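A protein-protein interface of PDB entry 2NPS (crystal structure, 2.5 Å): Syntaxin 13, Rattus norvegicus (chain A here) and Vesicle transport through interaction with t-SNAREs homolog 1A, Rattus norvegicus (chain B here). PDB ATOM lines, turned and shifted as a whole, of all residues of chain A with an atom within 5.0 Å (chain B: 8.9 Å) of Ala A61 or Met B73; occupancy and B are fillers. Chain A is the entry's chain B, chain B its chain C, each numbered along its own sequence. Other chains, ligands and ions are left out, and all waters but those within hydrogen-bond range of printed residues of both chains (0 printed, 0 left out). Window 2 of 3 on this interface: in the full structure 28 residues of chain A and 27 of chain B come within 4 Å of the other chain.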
ATOM      1  N   LEU A  57       5.303  -8.693  -9.210  1.00  0.00           N
ATOM      2  CA  LEU A  57       6.522  -9.456  -9.033  1.00  0.00           C
ATOM      3  C   LEU A  57       6.456 -10.305  -7.780  1.00  0.00           C
ATOM      4  O   LEU A  57       7.005 -11.398  -7.739  1.00  0.00           O
ATOM      5  CB  LEU A  57       7.716  -8.519  -8.976  1.00  0.00           C
ATOM      6  CG  LEU A  57       8.129  -7.967 -10.333  1.00  0.00           C
ATOM      7  CD1 LEU A  57       9.225  -6.956 -10.175  1.00  0.00           C
ATOM      8  CD2 LEU A  57       8.560  -9.097 -11.202  1.00  0.00           C
ATOM      9  N   GLN A  58       5.779  -9.802  -6.756  1.00  0.00           N
ATOM     10  CA  GLN A  58       5.622 -10.562  -5.519  1.00  0.00           C
ATOM     11  C   GLN A  58       4.739 -11.762  -5.785  1.00  0.00           C
ATOM     12  O   GLN A  58       4.941 -12.833  -5.220  1.00  0.00           O
ATOM     13  CB  GLN A  58       4.969  -9.721  -4.446  1.00  0.00           C
ATOM     14  CG  GLN A  58       5.833  -8.605  -3.948  1.00  0.00           C
ATOM     15  CD  GLN A  58       5.267  -7.997  -2.698  1.00  0.00           C
ATOM     16  OE1 GLN A  58       5.511  -6.833  -2.394  1.00  0.00           O
ATOM     17  NE2 GLN A  58       4.516  -8.795  -1.948  1.00  0.00           N
ATOM     18  N   ARG A  59       3.750 -11.566  -6.642  1.00  0.00           N
ATOM     19  CA  ARG A  59       2.856 -12.640  -7.013  1.00  0.00           C
ATOM     20  C   ARG A  59       3.633 -13.640  -7.873  1.00  0.00           C
ATOM     21  O   ARG A  59       3.444 -14.844  -7.764  1.00  0.00           O
ATOM     22  CB  ARG A  59       1.687 -12.099  -7.813  1.00  0.00           C
ATOM     23  CG  ARG A  59       0.795 -11.164  -7.065  1.00  0.00           C
ATOM     24  CD  ARG A  59      -0.508 -11.047  -7.823  1.00  0.00           C
ATOM     25  NE  ARG A  59      -1.588 -10.552  -6.985  1.00  0.00           N
ATOM     26  CZ  ARG A  59      -1.699  -9.298  -6.562  1.00  0.00           C
ATOM     27  NH1 ARG A  59      -2.732  -8.950  -5.796  1.00  0.00           N
ATOM     28  NH2 ARG A  59      -0.794  -8.386  -6.908  1.00  0.00           N
ATOM     29  N   ALA A  60       4.507 -13.128  -8.735  1.00  0.00           N
ATOM     30  CA  ALA A  60       5.326 -13.986  -9.590  1.00  0.00           C
ATOM     31  C   ALA A  60       6.230 -14.824  -8.719  1.00  0.00           C
ATOM     32  O   ALA A  60       6.378 -16.018  -8.945  1.00  0.00           O
ATOM     33  CB  ALA A  60       6.165 -13.148 -10.544  1.00  0.00           C
ATOM     34  N   ALA A  61       6.831 -14.186  -7.717  1.00  0.00           N
ATOM     35  CA  ALA A  61       7.731 -14.876  -6.795  1.00  0.00           C
ATOM     36  C   ALA A  61       6.986 -15.986  -6.068  1.00  0.00           C
ATOM     37  O   ALA A  61       7.452 -17.114  -6.023  1.00  0.00           O
ATOM     38  CB  ALA A  61       8.325 -13.894  -5.797  1.00  0.00           C
ATOM     39  N   TYR A  62       5.825 -15.659  -5.507  1.00  0.00           N
ATOM     40  CA  TYR A  62       5.008 -16.633  -4.792  1.00  0.00           C
ATOM     41  C   TYR A  62       4.733 -17.857  -5.645  1.00  0.00           C
ATOM     42  O   TYR A  62       4.875 -18.987  -5.190  1.00  0.00           O
ATOM     43  CB  TYR A  62       3.666 -16.022  -4.403  1.00  0.00           C
ATOM     44  CG  TYR A  62       2.673 -17.044  -3.891  1.00  0.00           C
ATOM     45  CD1 TYR A  62       2.842 -17.643  -2.640  1.00  0.00           C
ATOM     46  CD2 TYR A  62       1.573 -17.426  -4.659  1.00  0.00           C
ATOM     47  CE1 TYR A  62       1.942 -18.604  -2.159  1.00  0.00           C
ATOM     48  CE2 TYR A  62       0.660 -18.393  -4.191  1.00  0.00           C
ATOM     49  CZ  TYR A  62       0.853 -18.971  -2.937  1.00  0.00           C
ATOM     50  OH  TYR A  62      -0.035 -19.907  -2.459  1.00  0.00           O
ATOM     51  N   TYR A  63       4.308 -17.616  -6.880  1.00  0.00           N
ATOM     52  CA  TYR A  63       3.995 -18.680  -7.813  1.00  0.00           C
ATOM     53  C   TYR A  63       5.238 -19.484  -8.140  1.00  0.00           C
ATOM     54  O   TYR A  63       5.158 -20.673  -8.427  1.00  0.00           O
ATOM     55  CB  TYR A  63       3.385 -18.090  -9.081  1.00  0.00           C
ATOM     56  CG  TYR A  63       1.987 -17.547  -8.881  1.00  0.00           C
ATOM     57  CD1 TYR A  63       1.498 -16.503  -9.667  1.00  0.00           C
ATOM     58  CD2 TYR A  63       1.144 -18.075  -7.891  1.00  0.00           C
ATOM     59  CE1 TYR A  63       0.200 -15.990  -9.469  1.00  0.00           C
ATOM     60  CE2 TYR A  63      -0.156 -17.575  -7.684  1.00  0.00           C
ATOM     61  CZ  TYR A  63      -0.619 -16.534  -8.474  1.00  0.00           C
ATOM     62  OH  TYR A  63      -1.891 -16.036  -8.263  1.00  0.00           O
ATOM     63  N   GLN A  64       6.397 -18.846  -8.082  1.00  0.00           N
ATOM     64  CA  GLN A  64       7.618 -19.562  -8.377  1.00  0.00           C
ATOM     65  C   GLN A  64       7.875 -20.616  -7.300  1.00  0.00           C
ATOM     66  O   GLN A  64       8.259 -21.743  -7.604  1.00  0.00           O
ATOM     67  CB  GLN A  64       8.795 -18.598  -8.473  1.00  0.00           C
ATOM     68  CG  GLN A  64      10.077 -19.260  -8.920  1.00  0.00           C
ATOM     69  CD  GLN A  64      11.206 -18.278  -9.074  1.00  0.00           C
ATOM     70  OE1 GLN A  64      11.498 -17.497  -8.169  1.00  0.00           O
ATOM     71  NE2 GLN A  64      11.854 -18.312 -10.224  1.00  0.00           N
ATOM     72  N   LYS A  65       7.660 -20.253  -6.040  1.00  0.00           N
ATOM     73  CA  LYS A  65       7.854 -21.187  -4.935  1.00  0.00           C
ATOM     74  C   LYS A  65       6.665 -22.143  -4.849  1.00  0.00           C
ATOM     75  O   LYS A  65       6.826 -23.316  -4.516  1.00  0.00           O
ATOM     76  CB  LYS A  65       8.013 -20.441  -3.605  1.00  0.00           C
ATOM     77  CG  LYS A  65       9.299 -19.643  -3.473  1.00  0.00           C
ATOM     78  CD  LYS A  65       9.337 -18.829  -2.190  1.00  0.00           C
ATOM     79  N   SER B  66      11.432  -4.048  -6.209  1.00  0.00           N
ATOM     80  CA  SER B  66      11.342  -4.933  -7.366  1.00  0.00           C
ATOM     81  C   SER B  66      12.686  -5.603  -7.632  1.00  0.00           C
ATOM     82  O   SER B  66      12.758  -6.774  -7.997  1.00  0.00           O
ATOM     83  CB  SER B  66      10.883  -4.150  -8.604  1.00  0.00           C
ATOM     84  OG  SER B  66       9.538  -3.721  -8.477  1.00  0.00           O
ATOM     85  N   SER B  67      13.757  -4.852  -7.437  1.00  0.00           N
ATOM     86  CA  SER B  67      15.098  -5.384  -7.617  1.00  0.00           C
ATOM     87  C   SER B  67      15.359  -6.495  -6.618  1.00  0.00           C
ATOM     88  O   SER B  67      15.883  -7.539  -6.972  1.00  0.00           O
ATOM     89  CB  SER B  67      16.135  -4.290  -7.422  1.00  0.00           C
ATOM     90  OG  SER B  67      17.440  -4.828  -7.533  1.00  0.00           O
ATOM     91  N   ARG B  68      15.006  -6.272  -5.362  1.00  0.00           N
ATOM     92  CA  ARG B  68      15.195  -7.318  -4.375  1.00  0.00           C
ATOM     93  C   ARG B  68      14.345  -8.544  -4.767  1.00  0.00           C
ATOM     94  O   ARG B  68      14.860  -9.657  -4.809  1.00  0.00           O
ATOM     95  CB  ARG B  68      14.848  -6.791  -2.975  1.00  0.00           C
ATOM     96  CG  ARG B  68      14.507  -7.853  -1.940  1.00  0.00           C
ATOM     97  CD  ARG B  68      14.815  -7.403  -0.497  1.00  0.00           C
ATOM     98  NE  ARG B  68      16.154  -7.825  -0.060  1.00  0.00           N
ATOM     99  CZ  ARG B  68      17.226  -7.033   0.007  1.00  0.00           C
ATOM    100  NH1 ARG B  68      18.396  -7.517   0.409  1.00  0.00           N
ATOM    101  NH2 ARG B  68      17.132  -5.745  -0.306  1.00  0.00           N
ATOM    102  N   ILE B  69      13.066  -8.350  -5.103  1.00  0.00           N
ATOM    103  CA  ILE B  69      12.200  -9.481  -5.474  1.00  0.00           C
ATOM    104  C   ILE B  69      12.769 -10.274  -6.636  1.00  0.00           C
ATOM    105  O   ILE B  69      12.743 -11.501  -6.626  1.00  0.00           O
ATOM    106  CB  ILE B  69      10.755  -9.028  -5.855  1.00  0.00           C
ATOM    107  CG1 ILE B  69      10.054  -8.436  -4.651  1.00  0.00           C
ATOM    108  CG2 ILE B  69       9.924 -10.204  -6.334  1.00  0.00           C
ATOM    109  CD1 ILE B  69       8.676  -7.964  -4.947  1.00  0.00           C
ATOM    110  N   LEU B  70      13.297  -9.571  -7.629  1.00  0.00           N
ATOM    111  CA  LEU B  70      13.856 -10.228  -8.808  1.00  0.00           C
ATOM    112  C   LEU B  70      15.082 -11.049  -8.496  1.00  0.00           C
ATOM    113  O   LEU B  70      15.274 -12.130  -9.040  1.00  0.00           O
ATOM    114  CB  LEU B  70      14.190  -9.200  -9.875  1.00  0.00           C
ATOM    115  CG  LEU B  70      12.964  -8.732 -10.645  1.00  0.00           C
ATOM    116  CD1 LEU B  70      13.390  -7.746 -11.697  1.00  0.00           C
ATOM    117  CD2 LEU B  70      12.245  -9.930 -11.278  1.00  0.00           C
ATOM    118  N   THR B  71      15.921 -10.512  -7.622  1.00  0.00           N
ATOM    119  CA  THR B  71      17.119 -11.203  -7.190  1.00  0.00           C
ATOM    120  C   THR B  71      16.656 -12.522  -6.584  1.00  0.00           C
ATOM    121  O   THR B  71      17.155 -13.596  -6.923  1.00  0.00           O
ATOM    122  CB  THR B  71      17.858 -10.416  -6.083  1.00  0.00           C
ATOM    123  OG1 THR B  71      18.384  -9.194  -6.615  1.00  0.00           O
ATOM    124  CG2 THR B  71      18.976 -11.242  -5.522  1.00  0.00           C
ATOM    125  N   GLY B  72      15.695 -12.408  -5.667  1.00  0.00           N
ATOM    126  CA  GLY B  72      15.144 -13.559  -4.981  1.00  0.00           C
ATOM    127  C   GLY B  72      14.612 -14.591  -5.943  1.00  0.00           C
ATOM    128  O   GLY B  72      14.754 -15.784  -5.709  1.00  0.00           O
ATOM    129  N   MET B  73      13.994 -14.143  -7.032  1.00  0.00           N
ATOM    130  CA  MET B  73      13.456 -15.072  -8.015  1.00  0.00           C
ATOM    131  C   MET B  73      14.604 -15.730  -8.749  1.00  0.00           C
ATOM    132  O   MET B  73      14.572 -16.934  -8.989  1.00  0.00           O
ATOM    133  CB  MET B  73      12.533 -14.351  -9.010  1.00  0.00           C
ATOM    134  CG  MET B  73      11.176 -13.934  -8.425  1.00  0.00           C
ATOM    135  SD  MET B  73      10.074 -13.228  -9.648  1.00  0.00           S
ATOM    136  CE  MET B  73       9.561 -14.639 -10.473  1.00  0.00           C
ATOM    137  N   LEU B  74      15.614 -14.929  -9.091  1.00  0.00           N
ATOM    138  CA  LEU B  74      16.818 -15.402  -9.782  1.00  0.00           C
ATOM    139  C   LEU B  74      17.491 -16.513  -8.989  1.00  0.00           C
ATOM    140  O   LEU B  74      18.142 -17.391  -9.555  1.00  0.00           O
ATOM    141  CB  LEU B  74      17.828 -14.264  -9.967  1.00  0.00           C
ATOM    142  CG  LEU B  74      17.590 -13.322 -11.140  1.00  0.00           C
ATOM    143  CD1 LEU B  74      18.525 -12.128 -11.074  1.00  0.00           C
ATOM    144  CD2 LEU B  74      17.802 -14.090 -12.432  1.00  0.00           C
ATOM    145  N   ARG B  75      17.349 -16.456  -7.671  1.00  0.00           N
ATOM    146  CA  ARG B  75      17.945 -17.465  -6.819  1.00  0.00           C
ATOM    147  C   ARG B  75      17.174 -18.763  -6.974  1.00  0.00           C
ATOM    148  O   ARG B  75      17.728 -19.766  -7.405  1.00  0.00           O
ATOM    149  CB  ARG B  75      17.934 -17.003  -5.362  1.00  0.00           C
ATOM    150  CG  ARG B  75      19.061 -17.595  -4.553  1.00  0.00           C
ATOM    151  CD  ARG B  75      19.173 -16.956  -3.190  1.00  0.00           C
ATOM    152  NE  ARG B  75      19.527 -15.546  -3.271  1.00  0.00           N
ATOM    153  CZ  ARG B  75      19.576 -14.738  -2.218  1.00  0.00           C
ATOM    154  NH1 ARG B  75      19.906 -13.465  -2.374  1.00  0.00           N
ATOM    155  NH2 ARG B  75      19.295 -15.207  -1.005  1.00  0.00           N
ATOM    156  N   ARG B  76      15.886 -18.734  -6.654  1.00  0.00           N
ATOM    157  CA  ARG B  76      15.056 -19.928  -6.758  1.00  0.00           C
ATOM    158  C   ARG B  76      14.973 -20.550  -8.159  1.00  0.00           C
ATOM    159  O   ARG B  76      14.423 -21.634  -8.331  1.00  0.00           O
ATOM    160  CB  ARG B  76      13.660 -19.628  -6.217  1.00  0.00           C
ATOM    161  N   ILE B  77      15.532 -19.878  -9.158  1.00  0.00           N
ATOM    162  CA  ILE B  77      15.527 -20.422 -10.516  1.00  0.00           C
ATOM    163  C   ILE B  77      16.622 -21.473 -10.659  1.00  0.00           C
ATOM    164  O   ILE B  77      16.554 -22.355 -11.517  1.00  0.00           O
ATOM    165  CB  ILE B  77      15.761 -19.327 -11.576  1.00  0.00           C
ATOM    166  N   ILE B  78      17.646 -21.353  -9.821  1.00  0.00           N
ATOM    167  CA  ILE B  78      18.747 -22.307  -9.821  1.00  0.00           C
ATOM    168  C   ILE B  78      18.407 -23.325  -8.747  1.00  0.00           C
ATOM    169  O   ILE B  78      19.287 -23.977  -8.201  1.00  0.00           O
ATOM    170  N   GLN B  79      17.116 -23.429  -8.437  1.00  0.00           N
ATOM    171  CA  GLN B  79      16.623 -24.364  -7.427  1.00  0.00           C
ATOM    172  C   GLN B  79      17.282 -24.105  -6.074  1.00  0.00           C
ATOM    173  O   GLN B  79      18.008 -23.094  -5.958  1.00  0.00           O
ATOM    174  CB  GLN B  79      16.880 -25.807  -7.878  1.00  0.00           C
ATOM    175  CG  GLN B  79      16.634 -26.042  -9.367  1.00  0.00           C
ATOM    176  CD  GLN B  79      15.291 -25.495  -9.835  1.00  0.00           C
ATOM    177  OE1 GLN B  79      14.547 -24.877  -9.063  1.00  0.00           O
ATOM    178  NE2 GLN B  79      14.977 -25.715 -11.108  1.00  0.00           N
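The side-chain amide oxygen (OE1) of Gln A64 sits close to the backbone carbonyl oxygen (O) of Met B73 (3.2 Å).
The backbone carbonyl oxygen (O) of Arg B76 lies close to the side-chain amide oxygen (OE1) of Gln B79 (3.3 Å).
Among the printed residues, merely in contact across the chains: Leu A57 with Ser B66, Leu A57 with Ile B69, Leu A57 with Leu B70, Gln A58 with Ile B69, Ala A60 with Met B73, Ala A61 with Met B73 and Gln A64 with Arg B76.
Of the printed residues of chain B, Leu A57 touches Ser B66 (3.6 Å), Ile B69 (3.5 Å) and Leu B70 (3.8 Å). Of the printed residues of chain B, Gln A58 touches Ile B69 (3.1 Å). Of the printed residues of chain B, Ala A60 touches Met B73. Ala A61 touches one residue of chain B. Printed residues of chain B within 4 Å of Gln A64: Met B73 (3.1 Å) and Arg B76 (3.6 Å). Of the printed residues of chain A, Ser B66 touches Leu A57 (3.6 Å). Printed residues of chain A within 4 Å of Leu B70: Leu A57 (3.8 Å). Of the printed residues of chain A, Met B73 touches Ala A60 (3.7 Å), Ala A61 (3.9 Å) and Gln A64 (3.1 Å). The nearest residue of chain B that does not touch Ala A61 is Ile B69 (4.1 Å). The nearest residue of chain A that does not touch Met B73 is Leu A57 (4.1 Å).
Of the 14 printed residues of chain B, 5 touch a printed residue of chain A. Hydrophobic or aromatic side chains of chain B that line the printed part of chain A: Ile B69, Leu B70 and Met B73. Hydrophobic or aromatic side chains of chain A within 4 Å of the printed part of chain B: Leu A57, Ala A60 and Ala A61.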
